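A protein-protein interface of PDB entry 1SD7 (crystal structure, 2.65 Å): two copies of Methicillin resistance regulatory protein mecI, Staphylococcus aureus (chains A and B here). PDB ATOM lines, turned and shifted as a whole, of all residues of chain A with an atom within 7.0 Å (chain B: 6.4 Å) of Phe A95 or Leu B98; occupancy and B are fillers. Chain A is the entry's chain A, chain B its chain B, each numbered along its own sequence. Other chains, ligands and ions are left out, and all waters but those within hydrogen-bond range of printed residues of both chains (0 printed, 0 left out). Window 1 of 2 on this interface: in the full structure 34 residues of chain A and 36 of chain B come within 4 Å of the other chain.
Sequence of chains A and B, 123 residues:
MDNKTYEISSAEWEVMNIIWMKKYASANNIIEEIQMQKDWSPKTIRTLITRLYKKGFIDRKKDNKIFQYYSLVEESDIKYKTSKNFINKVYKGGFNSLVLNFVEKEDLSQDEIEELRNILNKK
Hydrophobic or aromatic side chains of chain B within 4 Å of the printed part of chain A: Phe B86, Tyr B91, Phe B95, Leu B98, Phe B102, Val B103 and Leu B116. Printed residues of chain A that touch a printed residue of chain B: Lys A79, Tyr A80, Ser A83, Lys A84, Phe A86, Tyr A91, Phe A95, Asn A96, Leu A98 and Leu A120. Hydrophobic or aromatic side chains of chain A within 4 Å of the printed part of chain B: Tyr A80, Phe A86, Tyr A91, Phe A95, Leu A98 and Leu A120. Among the printed residues, Asp or Glu carboxylates within 4 Å of a Lys or Arg side-chain nitrogen of the other chain: Lys A84 with Glu B106.
O of Lys A79 lies within hydrogen-bond range of OH of Tyr B91 (3.3 Å). The backbone NH of Tyr A80 sits close to the side-chain amide oxygen of Asn B101, 3.3 Å away. The side-chain carboxylate (OE1) of Glu B106 is in hydrogen-bond range of the side-chain hydroxyl (OH) of Tyr A80 (2.5 Å). The side-chain carboxylate (OE1) of Glu B106 lies within salt-bridge range of the side-chain amino group (NZ) of Lys A84 (3.2 Å). OH of Tyr A91 sits at hydrogen-bond distance from OG of Ser B83, 2.6 Å away. The side-chain amide nitrogen (ND2) of Asn A96 is in hydrogen-bond range of the side-chain carboxylate (OE1) of Glu B112, 2.7 Å away. The side-chain hydroxyl of Ser A83 lies close to the side-chain hydroxyl of Tyr B91, at 2.4 Å.
Ser A83 touches Tyr B91, and with the chains exchanged Tyr A91 touches Ser B83. Ser A83 touches Leu B98, but with the chains exchanged Leu A98 does not touch Ser B83 (4.1 Å). Phe B86 touches its own counterpart, Phe A86. Phe A95 touches Leu B98, and with the chains exchanged Leu A98 touches Phe B95. Of the 21 pairs that touch across the chains among the printed residues, 7 have their exchanged pair printed and touching as well.
The backbone carbonyl oxygen (O) of Lys A79 sits at hydrogen-bond distance from the side-chain hydroxyl (OG) of Ser A83, at 3.3 Å. The side-chain amide oxygen of Asn A101 is in hydrogen-bond range of the side-chain hydroxyl of Tyr A91, at 2.6 Å.
OG of Ser A83 touches CE2 of Phe B86 (3.6 Å). OG of Ser A83 touches CD1 of Leu B98, at 3.7 Å. Lys A84 touches Phe B102. OG of Ser B83 touches CZ of Phe A86, at 3.7 Å. Phe A86 touches Phe B86. Phe A95 touches Leu B98. Leu B116 touches Phe A95. Asn A96 touches Leu B116. CD2 of Leu A98 touches CE1 of Phe B95, at 3.6 Å. Leu A120 touches Val B103 (CD2 to CG2, 3.9 Å).
Of chain B, only Leu B98 (3.7 Å), Phe B102 (3.3 Å) and Leu B116 (3.7 Å) come within 4 Å of Phe A95. Of chain A, only Ser A83 (3.7 Å) and Phe A95 (3.7 Å) come within 4 Å of Leu B98. Printed residues of chain A within 4 Å of Leu B116: Phe A95 (3.7 Å), Asn A96 (3.2 Å) and Leu A120 (3.9 Å). Printed residues of chain A within 4 Å of Phe B95: Leu A98 (3.6 Å). Of the printed residues of chain B, Phe A86 touches Ser B83 (3.7 Å) and Phe B86 (3.5 Å). Of the printed residues of chain A, Phe B102 touches Tyr A80, Lys A84 and Phe A95. Of the printed residues of chain B, Tyr A80 touches Asn B101 (3.2 Å), Phe B102 (3.7 Å) and Glu B106 (2.5 Å). Ser A97 touches none of the printed residues of chain B.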
ATOM      1  N   LYS A  79     -30.311   1.709  37.772  1.00  0.00           N
ATOM      2  CA  LYS A  79     -30.794   0.818  36.731  1.00  0.00           C
ATOM      3  C   LYS A  79     -29.600   0.058  36.147  1.00  0.00           C
ATOM      4  O   LYS A  79     -29.696  -1.131  35.853  1.00  0.00           O
ATOM      5  CB  LYS A  79     -31.582   1.578  35.648  1.00  0.00           C
ATOM      6  CG  LYS A  79     -32.898   2.152  36.191  1.00  0.00           C
ATOM      7  CD  LYS A  79     -33.827   2.558  35.080  1.00  0.00           C
ATOM      8  CE  LYS A  79     -35.069   3.185  35.646  1.00  0.00           C
ATOM      9  NZ  LYS A  79     -36.046   3.488  34.597  1.00  0.00           N
ATOM     10  N   TYR A  80     -28.463   0.731  36.004  1.00  0.00           N
ATOM     11  CA  TYR A  80     -27.282   0.062  35.473  1.00  0.00           C
ATOM     12  C   TYR A  80     -26.904  -1.081  36.412  1.00  0.00           C
ATOM     13  O   TYR A  80     -26.809  -2.248  35.994  1.00  0.00           O
ATOM     14  CB  TYR A  80     -26.116   1.029  35.359  1.00  0.00           C
ATOM     15  CG  TYR A  80     -24.825   0.334  35.030  1.00  0.00           C
ATOM     16  CD1 TYR A  80     -24.736  -0.525  33.940  1.00  0.00           C
ATOM     17  CD2 TYR A  80     -23.691   0.539  35.807  1.00  0.00           C
ATOM     18  CE1 TYR A  80     -23.542  -1.169  33.629  1.00  0.00           C
ATOM     19  CE2 TYR A  80     -22.502  -0.089  35.510  1.00  0.00           C
ATOM     20  CZ  TYR A  80     -22.426  -0.945  34.419  1.00  0.00           C
ATOM     21  OH  TYR A  80     -21.226  -1.569  34.139  1.00  0.00           O
ATOM     22  N   SER A  83     -29.269  -4.020  36.247  1.00  0.00           N
ATOM     23  CA  SER A  83     -29.054  -4.845  35.047  1.00  0.00           C
ATOM     24  C   SER A  83     -27.790  -5.683  35.237  1.00  0.00           C
ATOM     25  O   SER A  83     -27.755  -6.837  34.856  1.00  0.00           O
ATOM     26  CB  SER A  83     -28.918  -3.971  33.803  1.00  0.00           C
ATOM     27  OG  SER A  83     -30.138  -3.331  33.445  1.00  0.00           O
ATOM     28  N   LYS A  84     -26.751  -5.110  35.834  1.00  0.00           N
ATOM     29  CA  LYS A  84     -25.523  -5.867  36.075  1.00  0.00           C
ATOM     30  C   LYS A  84     -25.867  -7.115  36.893  1.00  0.00           C
ATOM     31  O   LYS A  84     -25.478  -8.226  36.523  1.00  0.00           O
ATOM     32  CB  LYS A  84     -24.502  -5.021  36.839  1.00  0.00           C
ATOM     33  CG  LYS A  84     -23.926  -3.865  36.044  1.00  0.00           C
ATOM     34  CD  LYS A  84     -22.529  -4.180  35.577  1.00  0.00           C
ATOM     35  CE  LYS A  84     -22.482  -5.469  34.762  1.00  0.00           C
ATOM     36  NZ  LYS A  84     -21.109  -5.734  34.238  1.00  0.00           N
ATOM     37  N   PHE A  86     -28.875  -8.548  37.345  1.00  0.00           N
ATOM     38  CA  PHE A  86     -29.740  -9.445  36.581  1.00  0.00           C
ATOM     39  C   PHE A  86     -28.942 -10.336  35.610  1.00  0.00           C
ATOM     40  O   PHE A  86     -29.144 -11.554  35.516  1.00  0.00           O
ATOM     41  CB  PHE A  86     -30.767  -8.622  35.815  1.00  0.00           C
ATOM     42  CG  PHE A  86     -31.549  -9.417  34.839  1.00  0.00           C
ATOM     43  CD1 PHE A  86     -32.517 -10.314  35.276  1.00  0.00           C
ATOM     44  CD2 PHE A  86     -31.255  -9.342  33.485  1.00  0.00           C
ATOM     45  CE1 PHE A  86     -33.164 -11.121  34.379  1.00  0.00           C
ATOM     46  CE2 PHE A  86     -31.897 -10.156  32.578  1.00  0.00           C
ATOM     47  CZ  PHE A  86     -32.847 -11.042  33.021  1.00  0.00           C
ATOM     48  N   ILE A  87     -28.040  -9.699  34.881  1.00  0.00           N
ATOM     49  CA  ILE A  87     -27.196 -10.377  33.926  1.00  0.00           C
ATOM     50  C   ILE A  87     -26.287 -11.375  34.635  1.00  0.00           C
ATOM     51  O   ILE A  87     -26.061 -12.487  34.160  1.00  0.00           O
ATOM     52  CB  ILE A  87     -26.362  -9.341  33.160  1.00  0.00           C
ATOM     53  CG1 ILE A  87     -27.312  -8.507  32.280  1.00  0.00           C
ATOM     54  CG2 ILE A  87     -25.245 -10.050  32.377  1.00  0.00           C
ATOM     55  CD1 ILE A  87     -26.649  -7.425  31.495  1.00  0.00           C
ATOM     56  N   TYR A  91     -27.683 -14.986  32.836  1.00  0.00           N
ATOM     57  CA  TYR A  91     -26.821 -15.382  31.720  1.00  0.00           C
ATOM     58  C   TYR A  91     -25.384 -15.736  32.110  1.00  0.00           C
ATOM     59  O   TYR A  91     -24.837 -15.207  33.070  1.00  0.00           O
ATOM     60  CB  TYR A  91     -26.812 -14.269  30.679  1.00  0.00           C
ATOM     61  CG  TYR A  91     -28.169 -14.029  30.068  1.00  0.00           C
ATOM     62  CD1 TYR A  91     -28.585 -14.756  28.958  1.00  0.00           C
ATOM     63  CD2 TYR A  91     -29.050 -13.105  30.622  1.00  0.00           C
ATOM     64  CE1 TYR A  91     -29.839 -14.569  28.412  1.00  0.00           C
ATOM     65  CE2 TYR A  91     -30.314 -12.907  30.079  1.00  0.00           C
ATOM     66  CZ  TYR A  91     -30.699 -13.641  28.975  1.00  0.00           C
ATOM     67  OH  TYR A  91     -31.922 -13.427  28.400  1.00  0.00           O
ATOM     68  N   GLY A  93     -22.741 -15.447  29.935  1.00  0.00           N
ATOM     69  CA  GLY A  93     -21.910 -14.883  28.882  1.00  0.00           C
ATOM     70  C   GLY A  93     -21.902 -13.363  28.936  1.00  0.00           C
ATOM     71  O   GLY A  93     -21.491 -12.681  27.987  1.00  0.00           O
ATOM     72  N   GLY A  94     -22.355 -12.840  30.073  1.00  0.00           N
ATOM     73  CA  GLY A  94     -22.420 -11.415  30.278  1.00  0.00           C
ATOM     74  C   GLY A  94     -23.437 -10.805  29.343  1.00  0.00           C
ATOM     75  O   GLY A  94     -24.187 -11.520  28.676  1.00  0.00           O
ATOM     76  N   PHE A  95     -23.440  -9.477  29.303  1.00  0.00           N
ATOM     77  CA  PHE A  95     -24.316  -8.682  28.468  1.00  0.00           C
ATOM     78  C   PHE A  95     -24.458  -9.188  27.017  1.00  0.00           C
ATOM     79  O   PHE A  95     -25.560  -9.178  26.443  1.00  0.00           O
ATOM     80  CB  PHE A  95     -23.802  -7.247  28.477  1.00  0.00           C
ATOM     81  CG  PHE A  95     -24.650  -6.299  27.718  1.00  0.00           C
ATOM     82  CD1 PHE A  95     -25.888  -5.919  28.203  1.00  0.00           C
ATOM     83  CD2 PHE A  95     -24.206  -5.770  26.516  1.00  0.00           C
ATOM     84  CE1 PHE A  95     -26.681  -5.022  27.500  1.00  0.00           C
ATOM     85  CE2 PHE A  95     -24.992  -4.863  25.797  1.00  0.00           C
ATOM     86  CZ  PHE A  95     -26.230  -4.492  26.291  1.00  0.00           C
ATOM     87  N   ASN A  96     -23.348  -9.617  26.423  1.00  0.00           N
ATOM     88  CA  ASN A  96     -23.365 -10.124  25.060  1.00  0.00           C
ATOM     89  C   ASN A  96     -24.350 -11.297  24.919  1.00  0.00           C
ATOM     90  O   ASN A  96     -25.130 -11.352  23.965  1.00  0.00           O
ATOM     91  CB  ASN A  96     -21.934 -10.496  24.624  1.00  0.00           C
ATOM     92  CG  ASN A  96     -21.200  -9.317  23.961  1.00  0.00           C
ATOM     93  OD1 ASN A  96     -21.451  -9.000  22.796  1.00  0.00           O
ATOM     94  ND2 ASN A  96     -20.317  -8.656  24.708  1.00  0.00           N
ATOM     95  N   SER A  97     -24.334 -12.217  25.873  1.00  0.00           N
ATOM     96  CA  SER A  97     -25.263 -13.334  25.864  1.00  0.00           C
ATOM     97  C   SER A  97     -26.719 -12.863  25.836  1.00  0.00           C
ATOM     98  O   SER A  97     -27.515 -13.355  25.032  1.00  0.00           O
ATOM     99  CB  SER A  97     -25.061 -14.185  27.102  1.00  0.00           C
ATOM    100  OG  SER A  97     -24.077 -15.159  26.858  1.00  0.00           O
ATOM    101  N   LEU A  98     -27.070 -11.918  26.714  1.00  0.00           N
ATOM    102  CA  LEU A  98     -28.435 -11.415  26.769  1.00  0.00           C
ATOM    103  C   LEU A  98     -28.837 -10.807  25.444  1.00  0.00           C
ATOM    104  O   LEU A  98     -29.942 -11.039  24.966  1.00  0.00           O
ATOM    105  CB  LEU A  98     -28.596 -10.382  27.900  1.00  0.00           C
ATOM    106  CG  LEU A  98     -29.902  -9.611  28.147  1.00  0.00           C
ATOM    107  CD1 LEU A  98     -29.928  -9.123  29.568  1.00  0.00           C
ATOM    108  CD2 LEU A  98     -30.033  -8.423  27.234  1.00  0.00           C
ATOM    109  N   VAL A  99     -27.948 -10.042  24.828  1.00  0.00           N
ATOM    110  CA  VAL A  99     -28.306  -9.428  23.559  1.00  0.00           C
ATOM    111  C   VAL A  99     -28.509 -10.459  22.483  1.00  0.00           C
ATOM    112  O   VAL A  99     -29.420 -10.335  21.665  1.00  0.00           O
ATOM    113  CB  VAL A  99     -27.260  -8.439  23.058  1.00  0.00           C
ATOM    114  CG1 VAL A  99     -27.741  -7.839  21.746  1.00  0.00           C
ATOM    115  CG2 VAL A  99     -27.000  -7.367  24.110  1.00  0.00           C
ATOM    116  N   LEU A 100     -27.669 -11.485  22.485  1.00  0.00           N
ATOM    117  CA  LEU A 100     -27.776 -12.538  21.476  1.00  0.00           C
ATOM    118  C   LEU A 100     -29.074 -13.324  21.657  1.00  0.00           C
ATOM    119  O   LEU A 100     -29.725 -13.700  20.694  1.00  0.00           O
ATOM    120  CB  LEU A 100     -26.564 -13.482  21.562  1.00  0.00           C
ATOM    121  CG  LEU A 100     -26.530 -14.763  20.708  1.00  0.00           C
ATOM    122  CD1 LEU A 100     -26.536 -14.429  19.197  1.00  0.00           C
ATOM    123  CD2 LEU A 100     -25.282 -15.555  21.075  1.00  0.00           C
ATOM    124  N   ASN A 101     -29.446 -13.564  22.904  1.00  0.00           N
ATOM    125  CA  ASN A 101     -30.676 -14.294  23.207  1.00  0.00           C
ATOM    126  C   ASN A 101     -31.887 -13.452  22.809  1.00  0.00           C
ATOM    127  O   ASN A 101     -32.822 -13.935  22.172  1.00  0.00           O
ATOM    128  CB  ASN A 101     -30.672 -14.658  24.708  1.00  0.00           C
ATOM    129  CG  ASN A 101     -32.033 -15.011  25.257  1.00  0.00           C
ATOM    130  OD1 ASN A 101     -32.594 -14.258  26.041  1.00  0.00           O
ATOM    131  ND2 ASN A 101     -32.559 -16.159  24.872  1.00  0.00           N
ATOM    132  N   LEU A 120     -25.053   2.055  19.569  1.00  0.00           N
ATOM    133  CA  LEU A 120     -23.703   1.502  19.601  1.00  0.00           C
ATOM    134  C   LEU A 120     -22.727   2.469  18.885  1.00  0.00           C
ATOM    135  O   LEU A 120     -21.537   2.512  19.225  1.00  0.00           O
ATOM    136  CB  LEU A 120     -23.670   0.121  18.933  1.00  0.00           C
ATOM    137  CG  LEU A 120     -24.600  -0.994  19.415  1.00  0.00           C
ATOM    138  CD1 LEU A 120     -24.620  -2.094  18.388  1.00  0.00           C
ATOM    139  CD2 LEU A 120     -24.153  -1.534  20.731  1.00  0.00           C
ATOM    140  N   SER B  83     -35.993 -12.181  30.648  1.00  0.00           N
ATOM    141  CA  SER B  83     -35.467 -10.882  30.200  1.00  0.00           C
ATOM    142  C   SER B  83     -36.568  -9.869  29.871  1.00  0.00           C
ATOM    143  O   SER B  83     -36.442  -8.689  30.184  1.00  0.00           O
ATOM    144  CB  SER B  83     -34.569 -11.060  28.982  1.00  0.00           C
ATOM    145  OG  SER B  83     -33.282 -11.491  29.359  1.00  0.00           O
ATOM    146  N   PHE B  86     -37.899  -8.581  33.160  1.00  0.00           N
ATOM    147  CA  PHE B  86     -36.982  -7.723  33.884  1.00  0.00           C
ATOM    148  C   PHE B  86     -37.038  -6.322  33.307  1.00  0.00           C
ATOM    149  O   PHE B  86     -37.071  -5.332  34.046  1.00  0.00           O
ATOM    150  CB  PHE B  86     -35.572  -8.276  33.776  1.00  0.00           C
ATOM    151  CG  PHE B  86     -34.528  -7.383  34.351  1.00  0.00           C
ATOM    152  CD1 PHE B  86     -34.378  -7.266  35.727  1.00  0.00           C
ATOM    153  CD2 PHE B  86     -33.722  -6.616  33.511  1.00  0.00           C
ATOM    154  CE1 PHE B  86     -33.444  -6.400  36.263  1.00  0.00           C
ATOM    155  CE2 PHE B  86     -32.777  -5.736  34.028  1.00  0.00           C
ATOM    156  CZ  PHE B  86     -32.635  -5.625  35.409  1.00  0.00           C
ATOM    157  N   ILE B  87     -37.066  -6.273  31.976  1.00  0.00           N
ATOM    158  CA  ILE B  87     -37.100  -5.048  31.220  1.00  0.00           C
ATOM    159  C   ILE B  87     -38.396  -4.288  31.439  1.00  0.00           C
ATOM    160  O   ILE B  87     -38.396  -3.060  31.513  1.00  0.00           O
ATOM    161  CB  ILE B  87     -36.855  -5.352  29.707  1.00  0.00           C
ATOM    162  CG1 ILE B  87     -35.406  -5.803  29.503  1.00  0.00           C
ATOM    163  CG2 ILE B  87     -37.158  -4.112  28.852  1.00  0.00           C
ATOM    164  CD1 ILE B  87     -35.206  -6.591  28.253  1.00  0.00           C
ATOM    165  N   TYR B  91     -37.271  -0.942  33.111  1.00  0.00           N
ATOM    166  CA  TYR B  91     -37.191   0.080  32.063  1.00  0.00           C
ATOM    167  C   TYR B  91     -38.517   0.485  31.473  1.00  0.00           C
ATOM    168  O   TYR B  91     -39.417  -0.307  31.369  1.00  0.00           O
ATOM    169  CB  TYR B  91     -36.253  -0.405  30.956  1.00  0.00           C
ATOM    170  CG  TYR B  91     -34.831  -0.632  31.437  1.00  0.00           C
ATOM    171  CD1 TYR B  91     -33.912   0.405  31.440  1.00  0.00           C
ATOM    172  CD2 TYR B  91     -34.415  -1.876  31.915  1.00  0.00           C
ATOM    173  CE1 TYR B  91     -32.621   0.220  31.904  1.00  0.00           C
ATOM    174  CE2 TYR B  91     -33.118  -2.069  32.384  1.00  0.00           C
ATOM    175  CZ  TYR B  91     -32.233  -1.012  32.374  1.00  0.00           C
ATOM    176  OH  TYR B  91     -30.950  -1.169  32.835  1.00  0.00           O
ATOM    177  N   GLY B  94     -37.710   0.023  26.773  1.00  0.00           N
ATOM    178  CA  GLY B  94     -37.813  -1.355  26.340  1.00  0.00           C
ATOM    179  C   GLY B  94     -36.390  -1.868  26.291  1.00  0.00           C
ATOM    180  O   GLY B  94     -35.515  -1.288  26.937  1.00  0.00           O
ATOM    181  N   PHE B  95     -36.165  -2.955  25.562  1.00  0.00           N
ATOM    182  CA  PHE B  95     -34.835  -3.545  25.397  1.00  0.00           C
ATOM    183  C   PHE B  95     -33.859  -2.426  25.050  1.00  0.00           C
ATOM    184  O   PHE B  95     -32.697  -2.418  25.446  1.00  0.00           O
ATOM    185  CB  PHE B  95     -34.864  -4.531  24.243  1.00  0.00           C
ATOM    186  CG  PHE B  95     -33.562  -5.177  23.985  1.00  0.00           C
ATOM    187  CD1 PHE B  95     -32.992  -5.996  24.939  1.00  0.00           C
ATOM    188  CD2 PHE B  95     -32.876  -4.930  22.813  1.00  0.00           C
ATOM    189  CE1 PHE B  95     -31.756  -6.558  24.728  1.00  0.00           C
ATOM    190  CE2 PHE B  95     -31.645  -5.489  22.594  1.00  0.00           C
ATOM    191  CZ  PHE B  95     -31.079  -6.303  23.558  1.00  0.00           C
ATOM    192  N   ASN B  96     -34.394  -1.486  24.286  1.00  0.00           N
ATOM    193  CA  ASN B  96     -33.749  -0.264  23.804  1.00  0.00           C
ATOM    194  C   ASN B  96     -32.995   0.483  24.893  1.00  0.00           C
ATOM    195  O   ASN B  96     -31.815   0.808  24.753  1.00  0.00           O
ATOM    196  CB  ASN B  96     -34.845   0.676  23.306  1.00  0.00           C
ATOM    197  CG  ASN B  96     -34.507   1.367  22.024  1.00  0.00           C
ATOM    198  OD1 ASN B  96     -34.924   2.517  21.806  1.00  0.00           O
ATOM    199  ND2 ASN B  96     -33.783   0.679  21.143  1.00  0.00           N
ATOM    200  N   SER B  97     -33.726   0.804  25.955  1.00  0.00           N
ATOM    201  CA  SER B  97     -33.200   1.579  27.062  1.00  0.00           C
ATOM    202  C   SER B  97     -32.218   0.796  27.905  1.00  0.00           C
ATOM    203  O   SER B  97     -31.370   1.372  28.557  1.00  0.00           O
ATOM    204  CB  SER B  97     -34.337   2.065  27.953  1.00  0.00           C
ATOM    205  OG  SER B  97     -35.446   2.513  27.190  1.00  0.00           O
ATOM    206  N   LEU B  98     -32.344  -0.516  27.921  1.00  0.00           N
ATOM    207  CA  LEU B  98     -31.412  -1.280  28.709  1.00  0.00           C
ATOM    208  C   LEU B  98     -30.087  -1.234  27.941  1.00  0.00           C
ATOM    209  O   LEU B  98     -29.041  -0.973  28.530  1.00  0.00           O
ATOM    210  CB  LEU B  98     -31.919  -2.717  28.930  1.00  0.00           C
ATOM    211  CG  LEU B  98     -31.046  -3.647  29.773  1.00  0.00           C
ATOM    212  CD1 LEU B  98     -31.924  -4.681  30.481  1.00  0.00           C
ATOM    213  CD2 LEU B  98     -30.037  -4.351  28.885  1.00  0.00           C
ATOM    214  N   VAL B  99     -30.127  -1.462  26.630  1.00  0.00           N
ATOM    215  CA  VAL B  99     -28.891  -1.407  25.848  1.00  0.00           C
ATOM    216  C   VAL B  99     -28.375   0.043  25.907  1.00  0.00           C
ATOM    217  O   VAL B  99     -27.213   0.273  26.227  1.00  0.00           O
ATOM    218  CB  VAL B  99     -29.119  -1.882  24.378  1.00  0.00           C
ATOM    219  CG1 VAL B  99     -27.798  -1.803  23.560  1.00  0.00           C
ATOM    220  CG2 VAL B  99     -29.647  -3.320  24.397  1.00  0.00           C
ATOM    221  N   LEU B 100     -29.236   1.021  25.634  1.00  0.00           N
ATOM    222  CA  LEU B 100     -28.803   2.414  25.750  1.00  0.00           C
ATOM    223  C   LEU B 100     -28.064   2.633  27.063  1.00  0.00           C
ATOM    224  O   LEU B 100     -26.912   3.062  27.057  1.00  0.00           O
ATOM    225  CB  LEU B 100     -29.983   3.371  25.741  1.00  0.00           C
ATOM    226  CG  LEU B 100     -29.614   4.861  25.825  1.00  0.00           C
ATOM    227  CD1 LEU B 100     -28.722   5.212  24.650  1.00  0.00           C
ATOM    228  CD2 LEU B 100     -30.862   5.738  25.796  1.00  0.00           C
ATOM    229  N   ASN B 101     -28.741   2.321  28.176  1.00  0.00           N
ATOM    230  CA  ASN B 101     -28.203   2.488  29.529  1.00  0.00           C
ATOM    231  C   ASN B 101     -26.924   1.721  29.801  1.00  0.00           C
ATOM    232  O   ASN B 101     -26.024   2.229  30.486  1.00  0.00           O
ATOM    233  CB  ASN B 101     -29.273   2.111  30.595  1.00  0.00           C
ATOM    234  CG  ASN B 101     -28.794   2.342  32.064  1.00  0.00           C
ATOM    235  OD1 ASN B 101     -28.439   1.401  32.767  1.00  0.00           O
ATOM    236  ND2 ASN B 101     -28.797   3.593  32.512  1.00  0.00           N
ATOM    237  N   PHE B 102     -26.828   0.508  29.271  1.00  0.00           N
ATOM    238  CA  PHE B 102     -25.648  -0.316  29.501  1.00  0.00           C
ATOM    239  C   PHE B 102     -24.482   0.197  28.651  1.00  0.00           C
ATOM    240  O   PHE B 102     -23.348   0.311  29.131  1.00  0.00           O
ATOM    241  CB  PHE B 102     -25.995  -1.786  29.194  1.00  0.00           C
ATOM    242  CG  PHE B 102     -25.022  -2.777  29.754  1.00  0.00           C
ATOM    243  CD1 PHE B 102     -23.928  -3.190  29.011  1.00  0.00           C
ATOM    244  CD2 PHE B 102     -25.183  -3.277  31.044  1.00  0.00           C
ATOM    245  CE1 PHE B 102     -23.005  -4.102  29.547  1.00  0.00           C
ATOM    246  CE2 PHE B 102     -24.266  -4.183  31.590  1.00  0.00           C
ATOM    247  CZ  PHE B 102     -23.174  -4.595  30.840  1.00  0.00           C
ATOM    248  N   VAL B 103     -24.762   0.530  27.392  1.00  0.00           N
ATOM    249  CA  VAL B 103     -23.729   1.060  26.495  1.00  0.00           C
ATOM    250  C   VAL B 103     -23.273   2.462  26.973  1.00  0.00           C
ATOM    251  O   VAL B 103     -22.357   3.055  26.400  1.00  0.00           O
ATOM    252  CB  VAL B 103     -24.243   1.132  24.995  1.00  0.00           C
ATOM    253  CG1 VAL B 103     -23.294   1.943  24.133  1.00  0.00           C
ATOM    254  CG2 VAL B 103     -24.349  -0.262  24.413  1.00  0.00           C
ATOM    255  N   GLU B 106     -21.013   1.504  30.995  1.00  0.00           N
ATOM    256  CA  GLU B 106     -19.983   0.482  30.961  1.00  0.00           C
ATOM    257  C   GLU B 106     -19.057   0.948  29.850  1.00  0.00           C
ATOM    258  O   GLU B 106     -19.371   0.790  28.677  1.00  0.00           O
ATOM    259  CB  GLU B 106     -20.591  -0.887  30.635  1.00  0.00           C
ATOM    260  CG  GLU B 106     -19.567  -2.010  30.535  1.00  0.00           C
ATOM    261  CD  GLU B 106     -19.964  -3.246  31.324  1.00  0.00           C
ATOM    262  OE1 GLU B 106     -20.099  -3.150  32.559  1.00  0.00           O
ATOM    263  OE2 GLU B 106     -20.140  -4.319  30.709  1.00  0.00           O
ATOM    264  N   LEU B 108     -17.118  -0.044  28.026  1.00  0.00           N
ATOM    265  CA  LEU B 108     -17.088  -0.925  26.867  1.00  0.00           C
ATOM    266  C   LEU B 108     -15.991  -0.601  25.876  1.00  0.00           C
ATOM    267  O   LEU B 108     -15.990   0.467  25.262  1.00  0.00           O
ATOM    268  CB  LEU B 108     -18.436  -0.896  26.135  1.00  0.00           C
ATOM    269  CG  LEU B 108     -19.607  -1.719  26.690  1.00  0.00           C
ATOM    270  CD1 LEU B 108     -20.898  -1.211  26.101  1.00  0.00           C
ATOM    271  CD2 LEU B 108     -19.430  -3.193  26.364  1.00  0.00           C
ATOM    272  N   GLU B 112     -15.860  -4.575  21.973  1.00  0.00           N
ATOM    273  CA  GLU B 112     -17.105  -5.032  22.570  1.00  0.00           C
ATOM    274  C   GLU B 112     -18.226  -4.422  21.720  1.00  0.00           C
ATOM    275  O   GLU B 112     -19.193  -5.104  21.391  1.00  0.00           O
ATOM    276  CB  GLU B 112     -17.197  -4.559  24.024  1.00  0.00           C
ATOM    277  CG  GLU B 112     -16.533  -5.478  25.061  1.00  0.00           C
ATOM    278  CD  GLU B 112     -17.511  -6.486  25.690  1.00  0.00           C
ATOM    279  OE1 GLU B 112     -17.958  -7.415  24.978  1.00  0.00           O
ATOM    280  OE2 GLU B 112     -17.839  -6.339  26.897  1.00  0.00           O
ATOM    281  N   LEU B 116     -20.878  -6.528  19.755  1.00  0.00           N
ATOM    282  CA  LEU B 116     -22.308  -6.263  19.917  1.00  0.00           C
ATOM    283  C   LEU B 116     -22.918  -6.031  18.559  1.00  0.00           C
ATOM    284  O   LEU B 116     -24.073  -6.368  18.327  1.00  0.00           O
ATOM    285  CB  LEU B 116     -22.559  -5.045  20.818  1.00  0.00           C
ATOM    286  CG  LEU B 116     -22.343  -5.334  22.303  1.00  0.00           C
ATOM    287  CD1 LEU B 116     -22.549  -4.073  23.151  1.00  0.00           C
ATOM    288  CD2 LEU B 116     -23.317  -6.428  22.697  1.00  0.00           C
